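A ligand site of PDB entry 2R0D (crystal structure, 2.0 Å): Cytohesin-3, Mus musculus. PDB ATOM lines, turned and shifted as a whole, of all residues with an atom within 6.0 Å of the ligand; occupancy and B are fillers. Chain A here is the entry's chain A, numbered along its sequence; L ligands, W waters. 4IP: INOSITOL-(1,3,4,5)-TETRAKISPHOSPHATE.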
ATOM      1  N   LYS A 221       6.142   1.931 -22.996  1.00  0.00           N
ATOM      2  CA  LYS A 221       7.069   3.049 -23.006  1.00  0.00           C
ATOM      3  C   LYS A 221       6.675   4.132 -23.989  1.00  0.00           C
ATOM      4  O   LYS A 221       6.198   3.846 -25.092  1.00  0.00           O
ATOM      5  CB  LYS A 221       8.520   2.591 -23.220  1.00  0.00           C
ATOM      6  CG  LYS A 221       8.790   1.876 -24.542  1.00  0.00           C
ATOM      7  CD  LYS A 221      10.291   1.813 -24.837  1.00  0.00           C
ATOM      8  CE  LYS A 221      10.776   3.122 -25.490  1.00  0.00           C
ATOM      9  NZ  LYS A 221      10.157   3.304 -26.841  1.00  0.00           N
ATOM     10  N   LEU A 222       6.913   5.374 -23.588  1.00  0.00           N
ATOM     11  CA  LEU A 222       6.625   6.533 -24.420  1.00  0.00           C
ATOM     12  C   LEU A 222       7.824   6.855 -25.329  1.00  0.00           C
ATOM     13  O   LEU A 222       8.972   6.708 -24.898  1.00  0.00           O
ATOM     14  CB  LEU A 222       6.287   7.724 -23.533  1.00  0.00           C
ATOM     15  CG  LEU A 222       5.867   9.057 -24.172  1.00  0.00           C
ATOM     16  CD1 LEU A 222       4.591   8.876 -24.991  1.00  0.00           C
ATOM     17  CD2 LEU A 222       5.679  10.125 -23.086  1.00  0.00           C
ATOM     18  N   GLY A 223       7.538   7.275 -26.565  1.00  0.00           N
ATOM     19  CA  GLY A 223       8.563   7.586 -27.564  1.00  0.00           C
ATOM     20  C   GLY A 223       9.311   8.885 -27.300  1.00  0.00           C
ATOM     21  O   GLY A 223       8.969   9.624 -26.378  1.00  0.00           O
ATOM     22  N   GLY A 224      10.314   9.172 -28.121  1.00  0.00           N
ATOM     23  CA  GLY A 224      11.174  10.341 -27.938  1.00  0.00           C
ATOM     24  C   GLY A 224      10.586  11.537 -28.671  1.00  0.00           C
ATOM     25  O   GLY A 224       9.761  12.264 -28.127  1.00  0.00           O
ATOM     26  N   ARG A 225      11.004  11.727 -29.927  1.00  0.00           N
ATOM     27  CA  ARG A 225      10.418  12.789 -30.749  1.00  0.00           C
ATOM     28  C   ARG A 225       8.923  12.604 -30.925  1.00  0.00           C
ATOM     29  O   ARG A 225       8.144  13.538 -30.704  1.00  0.00           O
ATOM     30  CB  ARG A 225      11.118  12.906 -32.109  1.00  0.00           C
ATOM     31  CG  ARG A 225      12.577  13.353 -32.013  1.00  0.00           C
ATOM     32  CD  ARG A 225      13.241  13.392 -33.393  1.00  0.00           C
ATOM     33  NE  ARG A 225      12.754  14.507 -34.222  1.00  0.00           N
ATOM     34  CZ  ARG A 225      11.848  14.395 -35.196  1.00  0.00           C
ATOM     35  NH1 ARG A 225      11.319  13.204 -35.493  1.00  0.00           N
ATOM     36  NH2 ARG A 225      11.483  15.470 -35.881  1.00  0.00           N
ATOM     37  N   VAL A 226       8.524  11.400 -31.338  1.00  0.00           N
ATOM     38  CA  VAL A 226       7.119  11.045 -31.543  1.00  0.00           C
ATOM     39  C   VAL A 226       6.591  10.375 -30.283  1.00  0.00           C
ATOM     40  O   VAL A 226       7.040   9.294 -29.901  1.00  0.00           O
ATOM     41  CB  VAL A 226       6.931  10.117 -32.791  1.00  0.00           C
ATOM     42  CG1 VAL A 226       5.485   9.666 -32.919  1.00  0.00           C
ATOM     43  CG2 VAL A 226       7.390  10.806 -34.079  1.00  0.00           C
ATOM     44  N   LYS A 227       5.612  11.015 -29.642  1.00  0.00           N
ATOM     45  CA  LYS A 227       5.160  10.595 -28.331  1.00  0.00           C
ATOM     46  C   LYS A 227       4.090   9.511 -28.431  1.00  0.00           C
ATOM     47  O   LYS A 227       2.932   9.758 -28.128  1.00  0.00           O
ATOM     48  CB  LYS A 227       4.636  11.806 -27.517  1.00  0.00           C
ATOM     49  CG  LYS A 227       5.512  13.056 -27.597  1.00  0.00           C
ATOM     50  CD  LYS A 227       6.780  12.959 -26.776  1.00  0.00           C
ATOM     51  CE  LYS A 227       7.487  14.318 -26.680  1.00  0.00           C
ATOM     52  NZ  LYS A 227       8.238  14.729 -27.946  1.00  0.00           N
ATOM     53  N   THR A 228       4.503   8.320 -28.850  1.00  0.00           N
ATOM     54  CA  THR A 228       3.602   7.167 -28.888  1.00  0.00           C
ATOM     55  C   THR A 228       4.000   6.116 -27.842  1.00  0.00           C
ATOM     56  O   THR A 228       5.187   5.947 -27.520  1.00  0.00           O
ATOM     57  CB  THR A 228       3.554   6.522 -30.288  1.00  0.00           C
ATOM     58  OG1 THR A 228       4.883   6.358 -30.785  1.00  0.00           O
ATOM     59  CG2 THR A 228       2.767   7.405 -31.265  1.00  0.00           C
ATOM     60  N   TRP A 229       2.997   5.411 -27.317  1.00  0.00           N
ATOM     61  CA  TRP A 229       3.185   4.387 -26.305  1.00  0.00           C
ATOM     62  C   TRP A 229       3.313   3.008 -26.961  1.00  0.00           C
ATOM     63  O   TRP A 229       2.477   2.631 -27.773  1.00  0.00           O
ATOM     64  CB  TRP A 229       2.017   4.393 -25.321  1.00  0.00           C
ATOM     65  CG  TRP A 229       2.026   5.586 -24.390  1.00  0.00           C
ATOM     66  CD1 TRP A 229       1.377   6.775 -24.576  1.00  0.00           C
ATOM     67  CD2 TRP A 229       2.701   5.679 -23.137  1.00  0.00           C
ATOM     68  NE1 TRP A 229       1.612   7.615 -23.503  1.00  0.00           N
ATOM     69  CE2 TRP A 229       2.425   6.971 -22.609  1.00  0.00           C
ATOM     70  CE3 TRP A 229       3.525   4.811 -22.399  1.00  0.00           C
ATOM     71  CZ2 TRP A 229       2.946   7.411 -21.376  1.00  0.00           C
ATOM     72  CZ3 TRP A 229       4.047   5.256 -21.180  1.00  0.00           C
ATOM     73  CH2 TRP A 229       3.744   6.542 -20.685  1.00  0.00           C
ATOM     74  N   LYS A 230       4.382   2.280 -26.617  1.00  0.00           N
ATOM     75  CA  LYS A 230       4.663   0.944 -27.190  1.00  0.00           C
ATOM     76  C   LYS A 230       4.886  -0.106 -26.094  1.00  0.00           C
ATOM     77  O   LYS A 230       5.573   0.158 -25.104  1.00  0.00           O
ATOM     78  CB  LYS A 230       5.912   0.986 -28.078  1.00  0.00           C
ATOM     79  CG  LYS A 230       5.887   1.972 -29.236  1.00  0.00           C
ATOM     80  CD  LYS A 230       4.791   1.673 -30.247  1.00  0.00           C
ATOM     81  CE  LYS A 230       4.810   2.729 -31.356  1.00  0.00           C
ATOM     82  NZ  LYS A 230       3.650   2.606 -32.282  1.00  0.00           N
ATOM     83  N   ARG A 232       6.816  -3.057 -24.859  1.00  0.00           N
ATOM     84  CA  ARG A 232       8.172  -3.541 -25.125  1.00  0.00           C
ATOM     85  C   ARG A 232       8.622  -4.491 -24.035  1.00  0.00           C
ATOM     86  O   ARG A 232       8.171  -4.401 -22.889  1.00  0.00           O
ATOM     87  CB  ARG A 232       9.159  -2.380 -25.296  1.00  0.00           C
ATOM     88  CG  ARG A 232       8.846  -1.420 -26.480  1.00  0.00           C
ATOM     89  CD  ARG A 232       9.204  -2.052 -27.813  1.00  0.00           C
ATOM     90  NE  ARG A 232       8.876  -1.244 -28.989  1.00  0.00           N
ATOM     91  CZ  ARG A 232       7.832  -1.482 -29.790  1.00  0.00           C
ATOM     92  NH1 ARG A 232       7.003  -2.479 -29.539  1.00  0.00           N
ATOM     93  NH2 ARG A 232       7.629  -0.718 -30.853  1.00  0.00           N
ATOM     94  N   TYR A 243      15.618  -3.089 -24.431  1.00  0.00           N
ATOM     95  CA  TYR A 243      14.207  -3.360 -24.734  1.00  0.00           C
ATOM     96  C   TYR A 243      14.045  -3.916 -26.133  1.00  0.00           C
ATOM     97  O   TYR A 243      14.852  -3.646 -27.009  1.00  0.00           O
ATOM     98  CB  TYR A 243      13.292  -2.154 -24.461  1.00  0.00           C
ATOM     99  CG  TYR A 243      13.653  -0.860 -25.185  1.00  0.00           C
ATOM    100  CD1 TYR A 243      12.970  -0.479 -26.339  1.00  0.00           C
ATOM    101  CD2 TYR A 243      14.654  -0.024 -24.687  1.00  0.00           C
ATOM    102  CE1 TYR A 243      13.301   0.720 -27.008  1.00  0.00           C
ATOM    103  CE2 TYR A 243      14.982   1.166 -25.329  1.00  0.00           C
ATOM    104  CZ  TYR A 243      14.302   1.529 -26.496  1.00  0.00           C
ATOM    105  OH  TYR A 243      14.641   2.701 -27.128  1.00  0.00           O
ATOM    106  N   ARG A 253      15.518  -3.483 -29.686  1.00  0.00           N
ATOM    107  CA  ARG A 253      14.986  -2.249 -30.253  1.00  0.00           C
ATOM    108  C   ARG A 253      15.792  -1.037 -29.783  1.00  0.00           C
ATOM    109  O   ARG A 253      15.999  -0.080 -30.533  1.00  0.00           O
ATOM    110  CB  ARG A 253      13.497  -2.123 -29.876  1.00  0.00           C
ATOM    111  CG  ARG A 253      12.773  -0.902 -30.422  1.00  0.00           C
ATOM    112  CD  ARG A 253      12.851  -0.745 -31.941  1.00  0.00           C
ATOM    113  NE  ARG A 253      12.373  -1.925 -32.665  1.00  0.00           N
ATOM    114  CZ  ARG A 253      11.142  -2.077 -33.156  1.00  0.00           C
ATOM    115  NH1 ARG A 253      10.207  -1.150 -32.992  1.00  0.00           N
ATOM    116  NH2 ARG A 253      10.838  -3.201 -33.813  1.00  0.00           N
ATOM    117  N   GLY A 254      16.262  -1.077 -28.528  1.00  0.00           N
ATOM    118  CA  GLY A 254      17.099  -0.016 -27.979  1.00  0.00           C
ATOM    119  C   GLY A 254      17.879  -0.459 -26.751  1.00  0.00           C
ATOM    120  O   GLY A 254      17.567  -1.505 -26.157  1.00  0.00           O
ATOM    121  N   LYS A 291      19.143   3.133 -30.512  1.00  0.00           N
ATOM    122  CA  LYS A 291      17.958   2.384 -30.880  1.00  0.00           C
ATOM    123  C   LYS A 291      17.941   2.143 -32.388  1.00  0.00           C
ATOM    124  O   LYS A 291      18.702   2.783 -33.129  1.00  0.00           O
ATOM    125  CB  LYS A 291      16.676   3.091 -30.392  1.00  0.00           C
ATOM    126  CG  LYS A 291      16.576   4.586 -30.711  1.00  0.00           C
ATOM    127  CD  LYS A 291      16.193   4.840 -32.166  1.00  0.00           C
ATOM    128  CE  LYS A 291      15.388   6.117 -32.332  1.00  0.00           C
ATOM    129  NZ  LYS A 291      13.971   5.905 -31.914  1.00  0.00           N
ATOM    130  N   THR A 292      17.100   1.220 -32.839  1.00  0.00           N
ATOM    131  CA  THR A 292      16.989   0.913 -34.256  1.00  0.00           C
ATOM    132  C   THR A 292      15.764   1.559 -34.876  1.00  0.00           C
ATOM    133  O   THR A 292      14.725   1.699 -34.227  1.00  0.00           O
ATOM    134  CB  THR A 292      16.924  -0.603 -34.536  1.00  0.00           C
ATOM    135  OG1 THR A 292      15.765  -1.148 -33.893  1.00  0.00           O
ATOM    136  CG2 THR A 292      18.151  -1.306 -34.032  1.00  0.00           C
ATOM    137  N   GLU A 293      15.910   1.974 -36.124  1.00  0.00           N
ATOM    138  CA  GLU A 293      14.813   2.517 -36.928  1.00  0.00           C
ATOM    139  C   GLU A 293      14.201   1.411 -37.770  1.00  0.00           C
ATOM    140  O   GLU A 293      14.801   0.357 -37.937  1.00  0.00           O
ATOM    141  CB  GLU A 293      15.325   3.643 -37.834  1.00  0.00           C
ATOM    142  CG  GLU A 293      15.911   4.842 -37.098  1.00  0.00           C
ATOM    143  CD  GLU A 293      14.855   5.774 -36.521  1.00  0.00           C
ATOM    144  OE1 GLU A 293      13.687   5.344 -36.363  1.00  0.00           O
ATOM    145  OE2 GLU A 293      15.175   6.938 -36.231  1.00  0.00           O
ATOM    146  N   GLY A 301      19.349   7.817 -29.377  1.00  0.00           N
ATOM    147  CA  GLY A 301      18.050   8.157 -28.842  1.00  0.00           C
ATOM    148  C   GLY A 301      17.833   9.660 -28.807  1.00  0.00           C
ATOM    149  O   GLY A 301      18.790  10.435 -28.765  1.00  0.00           O
ATOM    150  N   ASN A 302      16.570  10.072 -28.798  1.00  0.00           N
ATOM    151  CA  ASN A 302      16.214  11.490 -28.733  1.00  0.00           C
ATOM    152  C   ASN A 302      15.516  11.874 -27.421  1.00  0.00           C
ATOM    153  O   ASN A 302      14.807  12.891 -27.370  1.00  0.00           O
ATOM    154  CB  ASN A 302      15.314  11.861 -29.926  1.00  0.00           C
ATOM    155  CG  ASN A 302      15.903  11.472 -31.268  1.00  0.00           C
ATOM    156  OD1 ASN A 302      17.026  11.859 -31.600  1.00  0.00           O
ATOM    157  ND2 ASN A 302      15.152  10.696 -32.052  1.00  0.00           N
ATOM    158  N   HIS A 303      15.674  11.063 -26.384  1.00  0.00           N
ATOM    159  CA  HIS A 303      14.911  11.230 -25.149  1.00  0.00           C
ATOM    160  C   HIS A 303      15.581  12.151 -24.165  1.00  0.00           C
ATOM    161  O   HIS A 303      16.768  11.983 -23.842  1.00  0.00           O
ATOM    162  CB  HIS A 303      14.724   9.885 -24.439  1.00  0.00           C
ATOM    163  CG  HIS A 303      13.684   9.003 -25.052  1.00  0.00           C
ATOM    164  ND1 HIS A 303      12.456   8.799 -24.485  1.00  0.00           N
ATOM    165  CD2 HIS A 303      13.720   8.241 -26.171  1.00  0.00           C
ATOM    166  CE1 HIS A 303      11.755   7.963 -25.234  1.00  0.00           C
ATOM    167  NE2 HIS A 303      12.500   7.598 -26.259  1.00  0.00           N
ATOM    168  N   TYR A 306      12.931   8.966 -20.224  1.00  0.00           N
ATOM    169  CA  TYR A 306      12.262   7.728 -20.635  1.00  0.00           C
ATOM    170  C   TYR A 306      11.108   7.470 -19.686  1.00  0.00           C
ATOM    171  O   TYR A 306      11.335   6.998 -18.576  1.00  0.00           O
ATOM    172  CB  TYR A 306      13.215   6.533 -20.619  1.00  0.00           C
ATOM    173  CG  TYR A 306      14.120   6.484 -21.820  1.00  0.00           C
ATOM    174  CD1 TYR A 306      13.703   5.869 -23.001  1.00  0.00           C
ATOM    175  CD2 TYR A 306      15.388   7.066 -21.787  1.00  0.00           C
ATOM    176  CE1 TYR A 306      14.532   5.835 -24.127  1.00  0.00           C
ATOM    177  CE2 TYR A 306      16.225   7.033 -22.890  1.00  0.00           C
ATOM    178  CZ  TYR A 306      15.777   6.412 -24.060  1.00  0.00           C
ATOM    179  OH  TYR A 306      16.595   6.396 -25.173  1.00  0.00           O
HETATM  180  C1  4IP L   1       8.239   5.625 -32.417  1.00  0.00           C
HETATM  181  O1  4IP L   1       6.872   5.961 -32.717  1.00  0.00           O
HETATM  182  C2  4IP L   1       8.238   4.678 -31.203  1.00  0.00           C
HETATM  183  O2  4IP L   1       7.567   5.287 -30.091  1.00  0.00           O
HETATM  184  C3  4IP L   1       9.671   4.342 -30.840  1.00  0.00           C
HETATM  185  O3  4IP L   1       9.688   3.337 -29.831  1.00  0.00           O
HETATM  186  C4  4IP L   1      10.471   5.576 -30.438  1.00  0.00           C
HETATM  187  O4  4IP L   1      11.839   5.200 -30.264  1.00  0.00           O
HETATM  188  C5  4IP L   1      10.438   6.647 -31.537  1.00  0.00           C
HETATM  189  O5  4IP L   1      11.010   7.858 -31.022  1.00  0.00           O
HETATM  190  C6  4IP L   1       9.024   6.904 -32.105  1.00  0.00           C
HETATM  191  O6  4IP L   1       9.152   7.677 -33.310  1.00  0.00           O
HETATM  192  P1  4IP L   1       6.060   5.275 -33.945  1.00  0.00           P
HETATM  193  O1P 4IP L   1       4.664   5.351 -33.444  1.00  0.00           O
HETATM  194  O2P 4IP L   1       6.372   6.172 -35.126  1.00  0.00           O
HETATM  195  O3P 4IP L   1       6.643   3.898 -34.109  1.00  0.00           O
HETATM  196  P3  4IP L   1      10.353   1.892 -30.111  1.00  0.00           P
HETATM  197  O4P 4IP L   1      11.795   2.167 -30.491  1.00  0.00           O
HETATM  198  O5P 4IP L   1       9.582   1.329 -31.295  1.00  0.00           O
HETATM  199  O6P 4IP L   1      10.185   1.166 -28.811  1.00  0.00           O
HETATM  200  P4  4IP L   1      12.582   5.060 -28.854  1.00  0.00           P
HETATM  201  O7P 4IP L   1      11.637   5.567 -27.785  1.00  0.00           O
HETATM  202  O8P 4IP L   1      13.843   5.869 -28.991  1.00  0.00           O
HETATM  203  O9P 4IP L   1      12.866   3.577 -28.713  1.00  0.00           O
HETATM  204  P5  4IP L   1      11.788   8.915 -31.957  1.00  0.00           P
HETATM  205  OPF 4IP L   1      12.685   8.145 -32.900  1.00  0.00           O
HETATM  206  OPG 4IP L   1      12.603   9.707 -30.962  1.00  0.00           O
HETATM  207  OPH 4IP L   1      10.651   9.649 -32.602  1.00  0.00           O
HETATM  208  O   HOH W   1      13.044   3.416 -32.723  1.00  0.00           O
HETATM  209  O   HOH W   2      14.362   8.447 -29.343  1.00  0.00           O
HETATM  210  O   HOH W   3       7.777   4.119 -27.422  1.00  0.00           O
HETATM  211  O   HOH W   4      11.856   6.974 -35.233  1.00  0.00           O
HETATM  212  O   HOH W   5       4.977   2.084 -35.484  1.00  0.00           O
HETATM  213  O   HOH W   6      14.742   8.888 -34.520  1.00  0.00           O
HETATM  214  O   HOH W   7      15.924   5.244 -27.355  1.00  0.00           O
HETATM  215  O   HOH W   8       8.450   2.078 -33.608  1.00  0.00           O
HETATM  216  O   HOH W   9      11.542  10.452 -35.028  1.00  0.00           O
HETATM  217  O   HOH W  10       5.321   5.434 -37.821  1.00  0.00           O
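An oxygen (O9P) of the ligand sits at hydrogen-bond distance from the side-chain hydroxyl (OH) of Tyr 243, 2.5 Å away. An oxygen (O7P) of the ligand lies within hydrogen-bond range of a ring nitrogen (NE2) of His 303 (2.7 Å). An oxygen (O6P) of the ligand lies within salt-bridge range of the guanidinium group (NE) of Arg 232 (2.7 Å). NZ of Lys 291 lies within salt-bridge range of OPF of the ligand (2.8 Å). An oxygen (OPG) of the ligand lies within hydrogen-bond range of the backbone NH (N) of Arg 225 (2.8 Å). An oxygen (O1) of the ligand is in hydrogen-bond range of the side-chain hydroxyl of Thr 228, 2.8 Å away. The side-chain amino group of Lys 221 is in salt-bridge range of an oxygen (O7P) of the ligand (2.9 Å). ND2 of Asn 302 is in hydrogen-bond range of OPG of the ligand (2.9 Å). The backbone NH of Val 226 lies within hydrogen-bond range of an oxygen (OPH) of the ligand (3.0 Å). The guanidinium group (NH1) of Arg 253 is in salt-bridge range of an oxygen (O5P) of the ligand. The side-chain amino group (NZ) of Lys 230 is in salt-bridge range of an oxygen (O1P) of the ligand, 3.1 Å away. An oxygen (O5) of the ligand lies within hydrogen-bond range of the backbone NH (N) of Gly 224, at 3.3 Å.
The backbone carbonyl oxygen (O) of Tyr 243 lies within hydrogen-bond range of the backbone NH (N) of Arg 253 (2.8 Å). The backbone carbonyl oxygen (O) of Gly 254 lies within hydrogen-bond range of the backbone NH (N) of Tyr 243 (3.0 Å). N of Gly 224 is in hydrogen-bond range of NE2 of His 303, 3.3 Å away. The side-chain amino group (NZ) of Lys 227 is in hydrogen-bond range of the backbone carbonyl oxygen (O) of Arg 225 (3.0 Å). O of Thr 228 sits at hydrogen-bond distance from N of Gly 223 (2.9 Å). The backbone carbonyl oxygen (O) of Lys 230 sits at hydrogen-bond distance from the backbone NH (N) of Lys 221, 2.8 Å away. N of Thr 292 is in hydrogen-bond range of O of Arg 253, at 2.9 Å. NZ of Lys 227 is in hydrogen-bond range of O of Gly 224.
Merely in contact with the ligand: Gly 223. Hydrophobic or aromatic side chains that line the ligand: Val 226, Tyr 243 and His 303. Within 4 Å of the ligand: Lys 221, Gly 223, Gly 224, Arg 225, Val 226, Thr 228, Lys 230, Arg 232, Tyr 243, Arg 253, Lys 291, Asn 302 and His 303.
Water W2 lies within hydrogen-bond range of O8P of the ligand (2.7 Å) and N of Asn 302 (2.8 Å). Water W9 bridges an oxygen (OPH) of the ligand (2.7 Å) and the guanidinium group (NH1) of Arg 225 (2.8 Å). Water W6 lies within hydrogen-bond range of OE2 of Glu 293 (2.6 Å), OPF of the ligand (2.7 Å) and ND2 of Asn 302 (3.1 Å). Water W4 bridges the side-chain carboxylate of Glu 293 and an oxygen (OPF) of the ligand. Water W1 lies within hydrogen-bond range of the side-chain amino group of Lys 291 (2.8 Å), the backbone carbonyl oxygen of Thr 292 (2.8 Å) and an oxygen (O4P) of the ligand (2.8 Å). Water W3 lies within hydrogen-bond range of the side-chain amino group of Lys 221 (2.6 Å), an oxygen (O2) of the ligand (2.9 Å), the backbone carbonyl oxygen of Thr 228 (3.2 Å) and the backbone NH of Gly 223 (3.3 Å).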
